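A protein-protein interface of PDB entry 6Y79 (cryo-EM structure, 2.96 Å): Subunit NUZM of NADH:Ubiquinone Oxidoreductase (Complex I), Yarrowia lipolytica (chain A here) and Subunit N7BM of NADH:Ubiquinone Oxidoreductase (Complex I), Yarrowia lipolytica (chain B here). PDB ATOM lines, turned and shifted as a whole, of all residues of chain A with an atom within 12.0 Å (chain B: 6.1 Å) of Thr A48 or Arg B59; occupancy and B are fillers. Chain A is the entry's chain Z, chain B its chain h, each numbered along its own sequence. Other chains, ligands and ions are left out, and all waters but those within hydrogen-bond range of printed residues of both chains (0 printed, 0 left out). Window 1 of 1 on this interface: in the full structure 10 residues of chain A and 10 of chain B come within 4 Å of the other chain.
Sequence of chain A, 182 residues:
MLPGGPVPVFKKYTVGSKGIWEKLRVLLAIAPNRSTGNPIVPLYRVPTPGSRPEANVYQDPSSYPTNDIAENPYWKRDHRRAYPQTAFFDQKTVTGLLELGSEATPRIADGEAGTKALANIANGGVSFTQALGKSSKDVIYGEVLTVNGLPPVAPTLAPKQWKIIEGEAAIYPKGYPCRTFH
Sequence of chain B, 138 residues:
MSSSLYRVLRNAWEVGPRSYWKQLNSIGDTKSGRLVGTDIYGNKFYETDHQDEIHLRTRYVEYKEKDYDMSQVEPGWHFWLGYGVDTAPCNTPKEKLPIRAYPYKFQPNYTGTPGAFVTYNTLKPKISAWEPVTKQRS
Among the printed residues, pairs that only touch across the chains: Ser A51 with Val B85 (3.2 Å), Pro A47 with Asp B86 (3.2 Å), Thr A48 with Tyr B83 (3.4 Å), Ser A51 with Gly B84 (3.7 Å), Thr A48 with Arg B59 (3.8 Å), Val A41 with Thr B58 (3.9 Å) and Pro A49 with Gly B84 (3.9 Å).
Of the 17 printed residues of chain B, 6 touch a printed residue of chain A. Hydrophobic or aromatic side chains of chain A within 4 Å of the printed part of chain B: Val A41 and Pro A47. Along chain A the printed residues that touch a printed residue of chain B span positions 41 to 51. Among the printed residues, 13 pairs touch across the chains.
O of Tyr B83 sits at hydrogen-bond distance from NH2 of Arg A45 (2.7 Å). OG1 of Thr A48 is in hydrogen-bond range of O of Gly B84, 2.7 Å away. The side-chain hydroxyl (OG1) of Thr A48 sits close to the backbone carbonyl oxygen (O) of Val B85. The side-chain hydroxyl (OG1) of Thr A48 lies within hydrogen-bond range of the side-chain carboxylate (OD1) of Asp B86 (3.1 Å). The backbone carbonyl oxygen of Gly B84 sits at hydrogen-bond distance from the backbone NH of Gly A50 (2.9 Å). The side-chain hydroxyl (OG) of Ser A51 is in hydrogen-bond range of the backbone NH (N) of Asp B86 (2.8 Å).
Of chain B, only Arg B59, Tyr B83, Gly B84, Val B85 and Asp B86 come within 4 Å of Thr A48. Of the printed residues of chain A, Arg B59 touches Thr A48 (3.8 Å). Thr B48 touches none of the printed residues of chain A. Thr B58 touches just one residue of chain A: Val A41 (3.9 Å). No residue of chain A comes within 4 Å of Trp B80. Leu B81 touches none of the printed residues of chain A. No residue of chain A comes within 4 Å of Gly B82. Tyr B83 touches two residues of chain A. Of chain A, only Thr A48, Pro A49, Gly A50 and Ser A51 come within 4 Å of Gly B84. Of the printed residues of chain A, Val B85 touches Thr A48 (3.2 Å) and Ser A51 (3.2 Å). Of the printed residues of chain A, Asp B86 touches Pro A47, Thr A48 and Ser A51. Of the printed residues of chain B, Gly A50 touches Gly B84. Of the printed residues of chain B, Pro A47 touches Asp B86 (3.2 Å). Printed residues of chain B within 4 Å of Arg A45: Tyr B83. Leu B56 touches none of the printed residues of chain A. The nearest residue of chain A that does not touch Arg B59 is Val A46 (7.0 Å).
The backbone NH (N) of Arg B57 lies within hydrogen-bond range of the side-chain hydroxyl (OH) of Tyr B83 (3.4 Å). OH of Tyr B83 sits at hydrogen-bond distance from N of Thr B58, 2.8 Å away. The guanidinium group (NE) of Arg B59 sits at hydrogen-bond distance from the backbone carbonyl oxygen (O) of Trp B80 (3.2 Å). The side-chain hydroxyl of Tyr B83 is in hydrogen-bond range of the backbone NH of Arg B59, 3.5 Å away. The guanidinium group (NH2) of Arg B59 sits at hydrogen-bond distance from the backbone carbonyl oxygen (O) of Val B85 (3.3 Å). O of Asp B86 lies within hydrogen-bond range of NE1 of Trp B80 (3.1 Å).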
ATOM      1  N   ILE A  40      10.075  -2.453   1.591  1.00  0.00           N
ATOM      2  CA  ILE A  40      10.710  -1.770   2.715  1.00  0.00           C
ATOM      3  C   ILE A  40       9.793  -0.657   3.201  1.00  0.00           C
ATOM      4  O   ILE A  40       9.510   0.290   2.461  1.00  0.00           O
ATOM      5  CB  ILE A  40      12.084  -1.216   2.323  1.00  0.00           C
ATOM      6  CG1 ILE A  40      13.015  -2.348   1.900  1.00  0.00           C
ATOM      7  CG2 ILE A  40      12.695  -0.468   3.484  1.00  0.00           C
ATOM      8  CD1 ILE A  40      14.357  -1.877   1.426  1.00  0.00           C
ATOM      9  N   VAL A  41       9.358  -0.757   4.454  1.00  0.00           N
ATOM     10  CA  VAL A  41       8.332   0.103   5.049  1.00  0.00           C
ATOM     11  C   VAL A  41       8.721   1.585   5.112  1.00  0.00           C
ATOM     12  O   VAL A  41       7.883   2.414   4.727  1.00  0.00           O
ATOM     13  CB  VAL A  41       7.919  -0.443   6.431  1.00  0.00           C
ATOM     14  CG1 VAL A  41       6.975   0.496   7.155  1.00  0.00           C
ATOM     15  CG2 VAL A  41       7.283  -1.782   6.266  1.00  0.00           C
ATOM     16  N   PRO A  42       9.934   2.006   5.533  1.00  0.00           N
ATOM     17  CA  PRO A  42      10.236   3.447   5.457  1.00  0.00           C
ATOM     18  C   PRO A  42      10.383   3.993   4.044  1.00  0.00           C
ATOM     19  O   PRO A  42      10.326   5.214   3.871  1.00  0.00           O
ATOM     20  CB  PRO A  42      11.554   3.571   6.232  1.00  0.00           C
ATOM     21  CG  PRO A  42      12.164   2.251   6.120  1.00  0.00           C
ATOM     22  CD  PRO A  42      11.014   1.330   6.287  1.00  0.00           C
ATOM     23  N   LEU A  43      10.560   3.143   3.031  1.00  0.00           N
ATOM     24  CA  LEU A  43      10.719   3.600   1.655  1.00  0.00           C
ATOM     25  C   LEU A  43       9.407   3.533   0.882  1.00  0.00           C
ATOM     26  O   LEU A  43       8.958   4.536   0.324  1.00  0.00           O
ATOM     27  CB  LEU A  43      11.784   2.765   0.936  1.00  0.00           C
ATOM     28  CG  LEU A  43      13.163   2.692   1.586  1.00  0.00           C
ATOM     29  CD1 LEU A  43      14.081   1.786   0.780  1.00  0.00           C
ATOM     30  CD2 LEU A  43      13.768   4.092   1.786  1.00  0.00           C
ATOM     31  N   TYR A  44       8.793   2.353   0.841  1.00  0.00           N
ATOM     32  CA  TYR A  44       7.586   2.103   0.061  1.00  0.00           C
ATOM     33  C   TYR A  44       6.406   2.813   0.705  1.00  0.00           C
ATOM     34  O   TYR A  44       5.973   2.437   1.800  1.00  0.00           O
ATOM     35  CB  TYR A  44       7.348   0.598  -0.028  1.00  0.00           C
ATOM     36  CG  TYR A  44       6.169   0.144  -0.866  1.00  0.00           C
ATOM     37  CD1 TYR A  44       6.313  -0.128  -2.216  1.00  0.00           C
ATOM     38  CD2 TYR A  44       4.928  -0.062  -0.291  1.00  0.00           C
ATOM     39  CE1 TYR A  44       5.238  -0.569  -2.974  1.00  0.00           C
ATOM     40  CE2 TYR A  44       3.858  -0.491  -1.039  1.00  0.00           C
ATOM     41  CZ  TYR A  44       4.013  -0.742  -2.376  1.00  0.00           C
ATOM     42  OH  TYR A  44       2.921  -1.177  -3.093  1.00  0.00           O
ATOM     43  N   ARG A  45       5.900   3.839   0.015  1.00  0.00           N
ATOM     44  CA  ARG A  45       4.722   4.629   0.378  1.00  0.00           C
ATOM     45  C   ARG A  45       4.887   5.301   1.748  1.00  0.00           C
ATOM     46  O   ARG A  45       4.186   5.010   2.720  1.00  0.00           O
ATOM     47  CB  ARG A  45       3.451   3.778   0.318  1.00  0.00           C
ATOM     48  CG  ARG A  45       2.188   4.597   0.307  1.00  0.00           C
ATOM     49  CD  ARG A  45       0.991   3.735   0.439  1.00  0.00           C
ATOM     50  NE  ARG A  45      -0.180   4.539   0.736  1.00  0.00           N
ATOM     51  CZ  ARG A  45      -1.404   4.055   0.709  1.00  0.00           C
ATOM     52  NH1 ARG A  45      -1.556   2.792   0.396  1.00  0.00           N
ATOM     53  NH2 ARG A  45      -2.452   4.817   0.984  1.00  0.00           N
ATOM     54  N   VAL A  46       5.879   6.183   1.801  1.00  0.00           N
ATOM     55  CA  VAL A  46       5.955   7.264   2.780  1.00  0.00           C
ATOM     56  C   VAL A  46       6.419   8.465   1.964  1.00  0.00           C
ATOM     57  O   VAL A  46       7.353   8.328   1.163  1.00  0.00           O
ATOM     58  CB  VAL A  46       6.902   6.946   3.956  1.00  0.00           C
ATOM     59  CG1 VAL A  46       7.332   8.216   4.675  1.00  0.00           C
ATOM     60  CG2 VAL A  46       6.239   6.035   4.970  1.00  0.00           C
ATOM     61  N   PRO A  47       5.789   9.639   2.078  1.00  0.00           N
ATOM     62  CA  PRO A  47       4.557   9.923   2.813  1.00  0.00           C
ATOM     63  C   PRO A  47       3.301   9.438   2.088  1.00  0.00           C
ATOM     64  O   PRO A  47       3.308   9.314   0.863  1.00  0.00           O
ATOM     65  CB  PRO A  47       4.579  11.446   2.929  1.00  0.00           C
ATOM     66  CG  PRO A  47       5.416  11.909   1.810  1.00  0.00           C
ATOM     67  CD  PRO A  47       6.470  10.876   1.662  1.00  0.00           C
ATOM     68  N   THR A  48       2.260   9.144   2.869  1.00  0.00           N
ATOM     69  CA  THR A  48       1.000   8.625   2.353  1.00  0.00           C
ATOM     70  C   THR A  48       0.352   9.647   1.413  1.00  0.00           C
ATOM     71  O   THR A  48       0.562  10.851   1.574  1.00  0.00           O
ATOM     72  CB  THR A  48       0.074   8.297   3.522  1.00  0.00           C
ATOM     73  OG1 THR A  48      -0.214   9.493   4.253  1.00  0.00           O
ATOM     74  CG2 THR A  48       0.733   7.292   4.449  1.00  0.00           C
ATOM     75  N   PRO A  49      -0.411   9.190   0.405  1.00  0.00           N
ATOM     76  CA  PRO A  49      -0.823  10.092  -0.694  1.00  0.00           C
ATOM     77  C   PRO A  49      -1.742  11.244  -0.312  1.00  0.00           C
ATOM     78  O   PRO A  49      -1.827  12.212  -1.076  1.00  0.00           O
ATOM     79  CB  PRO A  49      -1.532   9.144  -1.665  1.00  0.00           C
ATOM     80  CG  PRO A  49      -0.894   7.853  -1.435  1.00  0.00           C
ATOM     81  CD  PRO A  49      -0.647   7.783   0.033  1.00  0.00           C
ATOM     82  N   GLY A  50      -2.419  11.191   0.823  1.00  0.00           N
ATOM     83  CA  GLY A  50      -3.139  12.363   1.260  1.00  0.00           C
ATOM     84  C   GLY A  50      -2.284  13.356   2.008  1.00  0.00           C
ATOM     85  O   GLY A  50      -2.787  14.392   2.461  1.00  0.00           O
ATOM     86  N   SER A  51      -0.996  13.059   2.168  1.00  0.00           N
ATOM     87  CA  SER A  51      -0.074  13.913   2.889  1.00  0.00           C
ATOM     88  C   SER A  51       1.151  14.078   2.002  1.00  0.00           C
ATOM     89  O   SER A  51       2.130  13.353   2.141  1.00  0.00           O
ATOM     90  CB  SER A  51       0.293  13.310   4.217  1.00  0.00           C
ATOM     91  OG  SER A  51      -0.825  13.234   5.035  1.00  0.00           O
ATOM     92  N   ARG A  52       1.102  15.022   1.076  1.00  0.00           N
ATOM     93  CA  ARG A  52       2.210  15.237   0.176  1.00  0.00           C
ATOM     94  C   ARG A  52       2.539  16.722   0.122  1.00  0.00           C
ATOM     95  O   ARG A  52       1.632  17.552  -0.065  1.00  0.00           O
ATOM     96  CB  ARG A  52       1.874  14.698  -1.225  1.00  0.00           C
ATOM     97  CG  ARG A  52       1.722  13.178  -1.300  1.00  0.00           C
ATOM     98  CD  ARG A  52       3.045  12.433  -1.141  1.00  0.00           C
ATOM     99  NE  ARG A  52       3.996  12.746  -2.199  1.00  0.00           N
ATOM    100  CZ  ARG A  52       5.161  12.131  -2.369  1.00  0.00           C
ATOM    101  NH1 ARG A  52       5.519  11.156  -1.556  1.00  0.00           N
ATOM    102  NH2 ARG A  52       5.968  12.479  -3.360  1.00  0.00           N
ATOM    103  N   PRO A  53       3.812  17.096   0.275  1.00  0.00           N
ATOM    104  CA  PRO A  53       4.202  18.491   0.040  1.00  0.00           C
ATOM    105  C   PRO A  53       4.106  18.906  -1.420  1.00  0.00           C
ATOM    106  O   PRO A  53       4.078  20.113  -1.697  1.00  0.00           O
ATOM    107  CB  PRO A  53       5.651  18.535   0.538  1.00  0.00           C
ATOM    108  CG  PRO A  53       6.135  17.132   0.411  1.00  0.00           C
ATOM    109  CD  PRO A  53       4.945  16.267   0.724  1.00  0.00           C
ATOM    110  N   GLU A  54       4.050  17.950  -2.355  1.00  0.00           N
ATOM    111  CA  GLU A  54       3.947  18.276  -3.770  1.00  0.00           C
ATOM    112  C   GLU A  54       2.539  18.683  -4.170  1.00  0.00           C
ATOM    113  O   GLU A  54       2.355  19.239  -5.253  1.00  0.00           O
ATOM    114  CB  GLU A  54       4.378  17.088  -4.621  1.00  0.00           C
ATOM    115  CG  GLU A  54       5.869  16.775  -4.609  1.00  0.00           C
ATOM    116  CD  GLU A  54       6.199  15.688  -3.600  1.00  0.00           C
ATOM    117  OE1 GLU A  54       5.552  15.653  -2.530  1.00  0.00           O
ATOM    118  OE2 GLU A  54       7.086  14.854  -3.876  1.00  0.00           O
ATOM    119  N   ALA A  55       1.533  18.388  -3.343  1.00  0.00           N
ATOM    120  CA  ALA A  55       0.168  18.737  -3.711  1.00  0.00           C
ATOM    121  C   ALA A  55      -0.106  20.225  -3.567  1.00  0.00           C
ATOM    122  O   ALA A  55      -0.951  20.751  -4.285  1.00  0.00           O
ATOM    123  CB  ALA A  55      -0.836  17.944  -2.874  1.00  0.00           C
ATOM    124  N   ASN A  56       0.601  20.926  -2.687  1.00  0.00           N
ATOM    125  CA  ASN A  56       0.296  22.338  -2.506  1.00  0.00           C
ATOM    126  C   ASN A  56       0.999  23.212  -3.534  1.00  0.00           C
ATOM    127  O   ASN A  56       0.667  24.394  -3.659  1.00  0.00           O
ATOM    128  CB  ASN A  56       0.653  22.772  -1.086  1.00  0.00           C
ATOM    129  CG  ASN A  56       0.107  21.821  -0.037  1.00  0.00           C
ATOM    130  OD1 ASN A  56      -0.964  21.243  -0.203  1.00  0.00           O
ATOM    131  ND2 ASN A  56       0.849  21.651   1.050  1.00  0.00           N
ATOM    132  N   LYS B  31       0.885  -7.068  19.167  1.00  0.00           N
ATOM    133  CA  LYS B  31       1.297  -5.789  18.611  1.00  0.00           C
ATOM    134  C   LYS B  31       1.658  -4.816  19.726  1.00  0.00           C
ATOM    135  O   LYS B  31       0.974  -4.755  20.754  1.00  0.00           O
ATOM    136  CB  LYS B  31       0.182  -5.212  17.733  1.00  0.00           C
ATOM    137  CG  LYS B  31      -0.176  -6.039  16.509  1.00  0.00           C
ATOM    138  CD  LYS B  31       0.907  -5.949  15.466  1.00  0.00           C
ATOM    139  CE  LYS B  31       0.454  -5.118  14.292  1.00  0.00           C
ATOM    140  NZ  LYS B  31       1.499  -5.028  13.244  1.00  0.00           N
ATOM    141  N   TYR B  46      -3.045   2.815  17.551  1.00  0.00           N
ATOM    142  CA  TYR B  46      -1.637   2.577  17.813  1.00  0.00           C
ATOM    143  C   TYR B  46      -0.850   2.566  16.515  1.00  0.00           C
ATOM    144  O   TYR B  46      -1.363   2.189  15.459  1.00  0.00           O
ATOM    145  CB  TYR B  46      -1.421   1.261  18.556  1.00  0.00           C
ATOM    146  CG  TYR B  46      -2.002   1.224  19.947  1.00  0.00           C
ATOM    147  CD1 TYR B  46      -1.267   1.662  21.034  1.00  0.00           C
ATOM    148  CD2 TYR B  46      -3.286   0.746  20.172  1.00  0.00           C
ATOM    149  CE1 TYR B  46      -1.792   1.635  22.303  1.00  0.00           C
ATOM    150  CE2 TYR B  46      -3.823   0.720  21.438  1.00  0.00           C
ATOM    151  CZ  TYR B  46      -3.070   1.162  22.501  1.00  0.00           C
ATOM    152  OH  TYR B  46      -3.595   1.133  23.772  1.00  0.00           O
ATOM    153  N   GLU B  47       0.409   2.981  16.621  1.00  0.00           N
ATOM    154  CA  GLU B  47       1.373   2.955  15.537  1.00  0.00           C
ATOM    155  C   GLU B  47       2.636   2.260  16.026  1.00  0.00           C
ATOM    156  O   GLU B  47       3.138   2.562  17.110  1.00  0.00           O
ATOM    157  CB  GLU B  47       1.683   4.378  15.057  1.00  0.00           C
ATOM    158  CG  GLU B  47       2.608   4.445  13.874  1.00  0.00           C
ATOM    159  CD  GLU B  47       2.805   5.850  13.353  1.00  0.00           C
ATOM    160  OE1 GLU B  47       2.241   6.799  13.942  1.00  0.00           O
ATOM    161  OE2 GLU B  47       3.521   6.008  12.343  1.00  0.00           O
ATOM    162  N   THR B  48       3.144   1.331  15.223  1.00  0.00           N
ATOM    163  CA  THR B  48       4.262   0.466  15.586  1.00  0.00           C
ATOM    164  C   THR B  48       5.475   0.839  14.751  1.00  0.00           C
ATOM    165  O   THR B  48       5.418   0.807  13.521  1.00  0.00           O
ATOM    166  CB  THR B  48       3.923  -1.000  15.340  1.00  0.00           C
ATOM    167  OG1 THR B  48       3.856  -1.216  13.929  1.00  0.00           O
ATOM    168  CG2 THR B  48       2.587  -1.321  15.941  1.00  0.00           C
ATOM    169  N   LEU B  56       1.669  -2.083   5.424  1.00  0.00           N
ATOM    170  CA  LEU B  56       0.261  -2.111   5.847  1.00  0.00           C
ATOM    171  C   LEU B  56       0.032  -2.835   7.174  1.00  0.00           C
ATOM    172  O   LEU B  56      -1.051  -3.365   7.409  1.00  0.00           O
ATOM    173  CB  LEU B  56      -0.667  -2.661   4.757  1.00  0.00           C
ATOM    174  CG  LEU B  56      -0.541  -2.167   3.316  1.00  0.00           C
ATOM    175  CD1 LEU B  56      -1.411  -3.019   2.413  1.00  0.00           C
ATOM    176  CD2 LEU B  56      -0.863  -0.659   3.142  1.00  0.00           C
ATOM    177  N   ARG B  57       1.011  -2.832   8.082  1.00  0.00           N
ATOM    178  CA  ARG B  57       0.806  -3.358   9.429  1.00  0.00           C
ATOM    179  C   ARG B  57       1.134  -2.356  10.525  1.00  0.00           C
ATOM    180  O   ARG B  57       0.964  -2.677  11.707  1.00  0.00           O
ATOM    181  CB  ARG B  57       1.643  -4.622   9.646  1.00  0.00           C
ATOM    182  CG  ARG B  57       1.398  -5.725   8.643  1.00  0.00           C
ATOM    183  CD  ARG B  57       0.053  -6.382   8.845  1.00  0.00           C
ATOM    184  NE  ARG B  57      -0.155  -6.823  10.219  1.00  0.00           N
ATOM    185  CZ  ARG B  57       0.218  -8.009  10.684  1.00  0.00           C
ATOM    186  NH1 ARG B  57      -0.015  -8.333  11.945  1.00  0.00           N
ATOM    187  NH2 ARG B  57       0.829  -8.869   9.885  1.00  0.00           N
ATOM    188  N   THR B  58       1.577  -1.151  10.163  1.00  0.00           N
ATOM    189  CA  THR B  58       2.142  -0.218  11.131  1.00  0.00           C
ATOM    190  C   THR B  58       1.072   0.336  12.071  1.00  0.00           C
ATOM    191  O   THR B  58       1.324   0.528  13.265  1.00  0.00           O
ATOM    192  CB  THR B  58       2.882   0.882  10.358  1.00  0.00           C
ATOM    193  OG1 THR B  58       4.051   0.321   9.752  1.00  0.00           O
ATOM    194  CG2 THR B  58       3.310   2.030  11.233  1.00  0.00           C
ATOM    195  N   ARG B  59      -0.144   0.534  11.576  1.00  0.00           N
ATOM    196  CA  ARG B  59      -1.189   1.212  12.328  1.00  0.00           C
ATOM    197  C   ARG B  59      -2.359   0.279  12.578  1.00  0.00           C
ATOM    198  O   ARG B  59      -2.698  -0.536  11.718  1.00  0.00           O
ATOM    199  CB  ARG B  59      -1.667   2.437  11.564  1.00  0.00           C
ATOM    200  CG  ARG B  59      -0.522   3.309  11.208  1.00  0.00           C
ATOM    201  CD  ARG B  59      -0.942   4.702  11.109  1.00  0.00           C
ATOM    202  NE  ARG B  59      -1.213   5.211   9.783  1.00  0.00           N
ATOM    203  CZ  ARG B  59      -0.283   5.812   9.058  1.00  0.00           C
ATOM    204  NH1 ARG B  59       0.950   5.914   9.533  1.00  0.00           N
ATOM    205  NH2 ARG B  59      -0.570   6.292   7.864  1.00  0.00           N
ATOM    206  N   TYR B  60      -2.989   0.413  13.744  1.00  0.00           N
ATOM    207  CA  TYR B  60      -4.139  -0.426  14.052  1.00  0.00           C
ATOM    208  C   TYR B  60      -5.015   0.225  15.111  1.00  0.00           C
ATOM    209  O   TYR B  60      -4.669   1.251  15.696  1.00  0.00           O
ATOM    210  CB  TYR B  60      -3.716  -1.836  14.488  1.00  0.00           C
ATOM    211  CG  TYR B  60      -2.902  -1.926  15.754  1.00  0.00           C
ATOM    212  CD1 TYR B  60      -1.525  -1.785  15.723  1.00  0.00           C
ATOM    213  CD2 TYR B  60      -3.509  -2.196  16.975  1.00  0.00           C
ATOM    214  CE1 TYR B  60      -0.785  -1.876  16.868  1.00  0.00           C
ATOM    215  CE2 TYR B  60      -2.771  -2.291  18.126  1.00  0.00           C
ATOM    216  CZ  TYR B  60      -1.407  -2.137  18.064  1.00  0.00           C
ATOM    217  OH  TYR B  60      -0.655  -2.228  19.210  1.00  0.00           O
ATOM    218  N   VAL B  61      -6.172  -0.391  15.336  1.00  0.00           N
ATOM    219  CA  VAL B  61      -7.150   0.048  16.323  1.00  0.00           C
ATOM    220  C   VAL B  61      -7.305  -1.048  17.369  1.00  0.00           C
ATOM    221  O   VAL B  61      -7.240  -2.240  17.051  1.00  0.00           O
ATOM    222  CB  VAL B  61      -8.498   0.400  15.645  1.00  0.00           C
ATOM    223  CG1 VAL B  61      -8.972  -0.706  14.760  1.00  0.00           C
ATOM    224  CG2 VAL B  61      -9.597   0.719  16.640  1.00  0.00           C
ATOM    225  N   TRP B  80      -7.071   7.979   8.467  1.00  0.00           N
ATOM    226  CA  TRP B  80      -5.730   7.766   8.996  1.00  0.00           C
ATOM    227  C   TRP B  80      -5.388   6.298   9.152  1.00  0.00           C
ATOM    228  O   TRP B  80      -4.248   5.901   8.882  1.00  0.00           O
ATOM    229  CB  TRP B  80      -5.606   8.480  10.336  1.00  0.00           C
ATOM    230  CG  TRP B  80      -4.235   8.404  10.930  1.00  0.00           C
ATOM    231  CD1 TRP B  80      -3.137   9.104  10.510  1.00  0.00           C
ATOM    232  CD2 TRP B  80      -3.805   7.599  12.022  1.00  0.00           C
ATOM    233  NE1 TRP B  80      -2.066   8.788  11.263  1.00  0.00           N
ATOM    234  CE2 TRP B  80      -2.440   7.863  12.205  1.00  0.00           C
ATOM    235  CE3 TRP B  80      -4.440   6.679  12.861  1.00  0.00           C
ATOM    236  CZ2 TRP B  80      -1.702   7.263  13.218  1.00  0.00           C
ATOM    237  CZ3 TRP B  80      -3.705   6.066  13.833  1.00  0.00           C
ATOM    238  CH2 TRP B  80      -2.349   6.333  13.986  1.00  0.00           C
ATOM    239  N   LEU B  81      -6.363   5.495   9.579  1.00  0.00           N
ATOM    240  CA  LEU B  81      -6.134   4.068   9.755  1.00  0.00           C
ATOM    241  C   LEU B  81      -5.849   3.378   8.426  1.00  0.00           C
ATOM    242  O   LEU B  81      -5.051   2.433   8.374  1.00  0.00           O
ATOM    243  CB  LEU B  81      -7.347   3.453  10.442  1.00  0.00           C
ATOM    244  CG  LEU B  81      -7.240   2.124  11.213  1.00  0.00           C
ATOM    245  CD1 LEU B  81      -8.258   2.143  12.316  1.00  0.00           C
ATOM    246  CD2 LEU B  81      -7.501   0.951  10.325  1.00  0.00           C
ATOM    247  N   GLY B  82      -6.452   3.853   7.352  1.00  0.00           N
ATOM    248  CA  GLY B  82      -6.239   3.314   6.034  1.00  0.00           C
ATOM    249  C   GLY B  82      -5.062   3.875   5.275  1.00  0.00           C
ATOM    250  O   GLY B  82      -4.984   3.673   4.064  1.00  0.00           O
ATOM    251  N   TYR B  83      -4.178   4.600   5.959  1.00  0.00           N
ATOM    252  CA  TYR B  83      -2.946   5.189   5.421  1.00  0.00           C
ATOM    253  C   TYR B  83      -3.238   6.238   4.366  1.00  0.00           C
ATOM    254  O   TYR B  83      -2.669   6.227   3.274  1.00  0.00           O
ATOM    255  CB  TYR B  83      -1.984   4.167   4.830  1.00  0.00           C
ATOM    256  CG  TYR B  83      -1.364   3.188   5.755  1.00  0.00           C
ATOM    257  CD1 TYR B  83      -1.644   3.174   7.110  1.00  0.00           C
ATOM    258  CD2 TYR B  83      -0.410   2.336   5.276  1.00  0.00           C
ATOM    259  CE1 TYR B  83      -1.071   2.263   7.926  1.00  0.00           C
ATOM    260  CE2 TYR B  83       0.194   1.452   6.078  1.00  0.00           C
ATOM    261  CZ  TYR B  83      -0.126   1.410   7.385  1.00  0.00           C
ATOM    262  OH  TYR B  83       0.518   0.497   8.145  1.00  0.00           O
ATOM    263  N   GLY B  84      -4.135   7.143   4.692  1.00  0.00           N
ATOM    264  CA  GLY B  84      -4.342   8.250   3.804  1.00  0.00           C
ATOM    265  C   GLY B  84      -3.480   9.410   4.249  1.00  0.00           C
ATOM    266  O   GLY B  84      -2.774  10.019   3.452  1.00  0.00           O
ATOM    267  N   VAL B  85      -3.529   9.740   5.519  1.00  0.00           N
ATOM    268  CA  VAL B  85      -2.857  10.919   6.023  1.00  0.00           C
ATOM    269  C   VAL B  85      -1.720  10.462   6.938  1.00  0.00           C
ATOM    270  O   VAL B  85      -1.692   9.309   7.385  1.00  0.00           O
ATOM    271  CB  VAL B  85      -3.913  11.822   6.699  1.00  0.00           C
ATOM    272  CG1 VAL B  85      -4.531  11.138   7.927  1.00  0.00           C
ATOM    273  CG2 VAL B  85      -3.359  13.216   7.067  1.00  0.00           C
ATOM    274  N   ASP B  86      -0.695  11.310   7.082  1.00  0.00           N
ATOM    275  CA  ASP B  86       0.351  11.019   8.056  1.00  0.00           C
ATOM    276  C   ASP B  86      -0.049  11.486   9.441  1.00  0.00           C
ATOM    277  O   ASP B  86       0.164  10.781  10.433  1.00  0.00           O
ATOM    278  CB  ASP B  86       1.679  11.684   7.690  1.00  0.00           C
ATOM    279  CG  ASP B  86       2.311  11.126   6.439  1.00  0.00           C
ATOM    280  OD1 ASP B  86       2.157   9.919   6.187  1.00  0.00           O
ATOM    281  OD2 ASP B  86       2.938  11.903   5.692  1.00  0.00           O
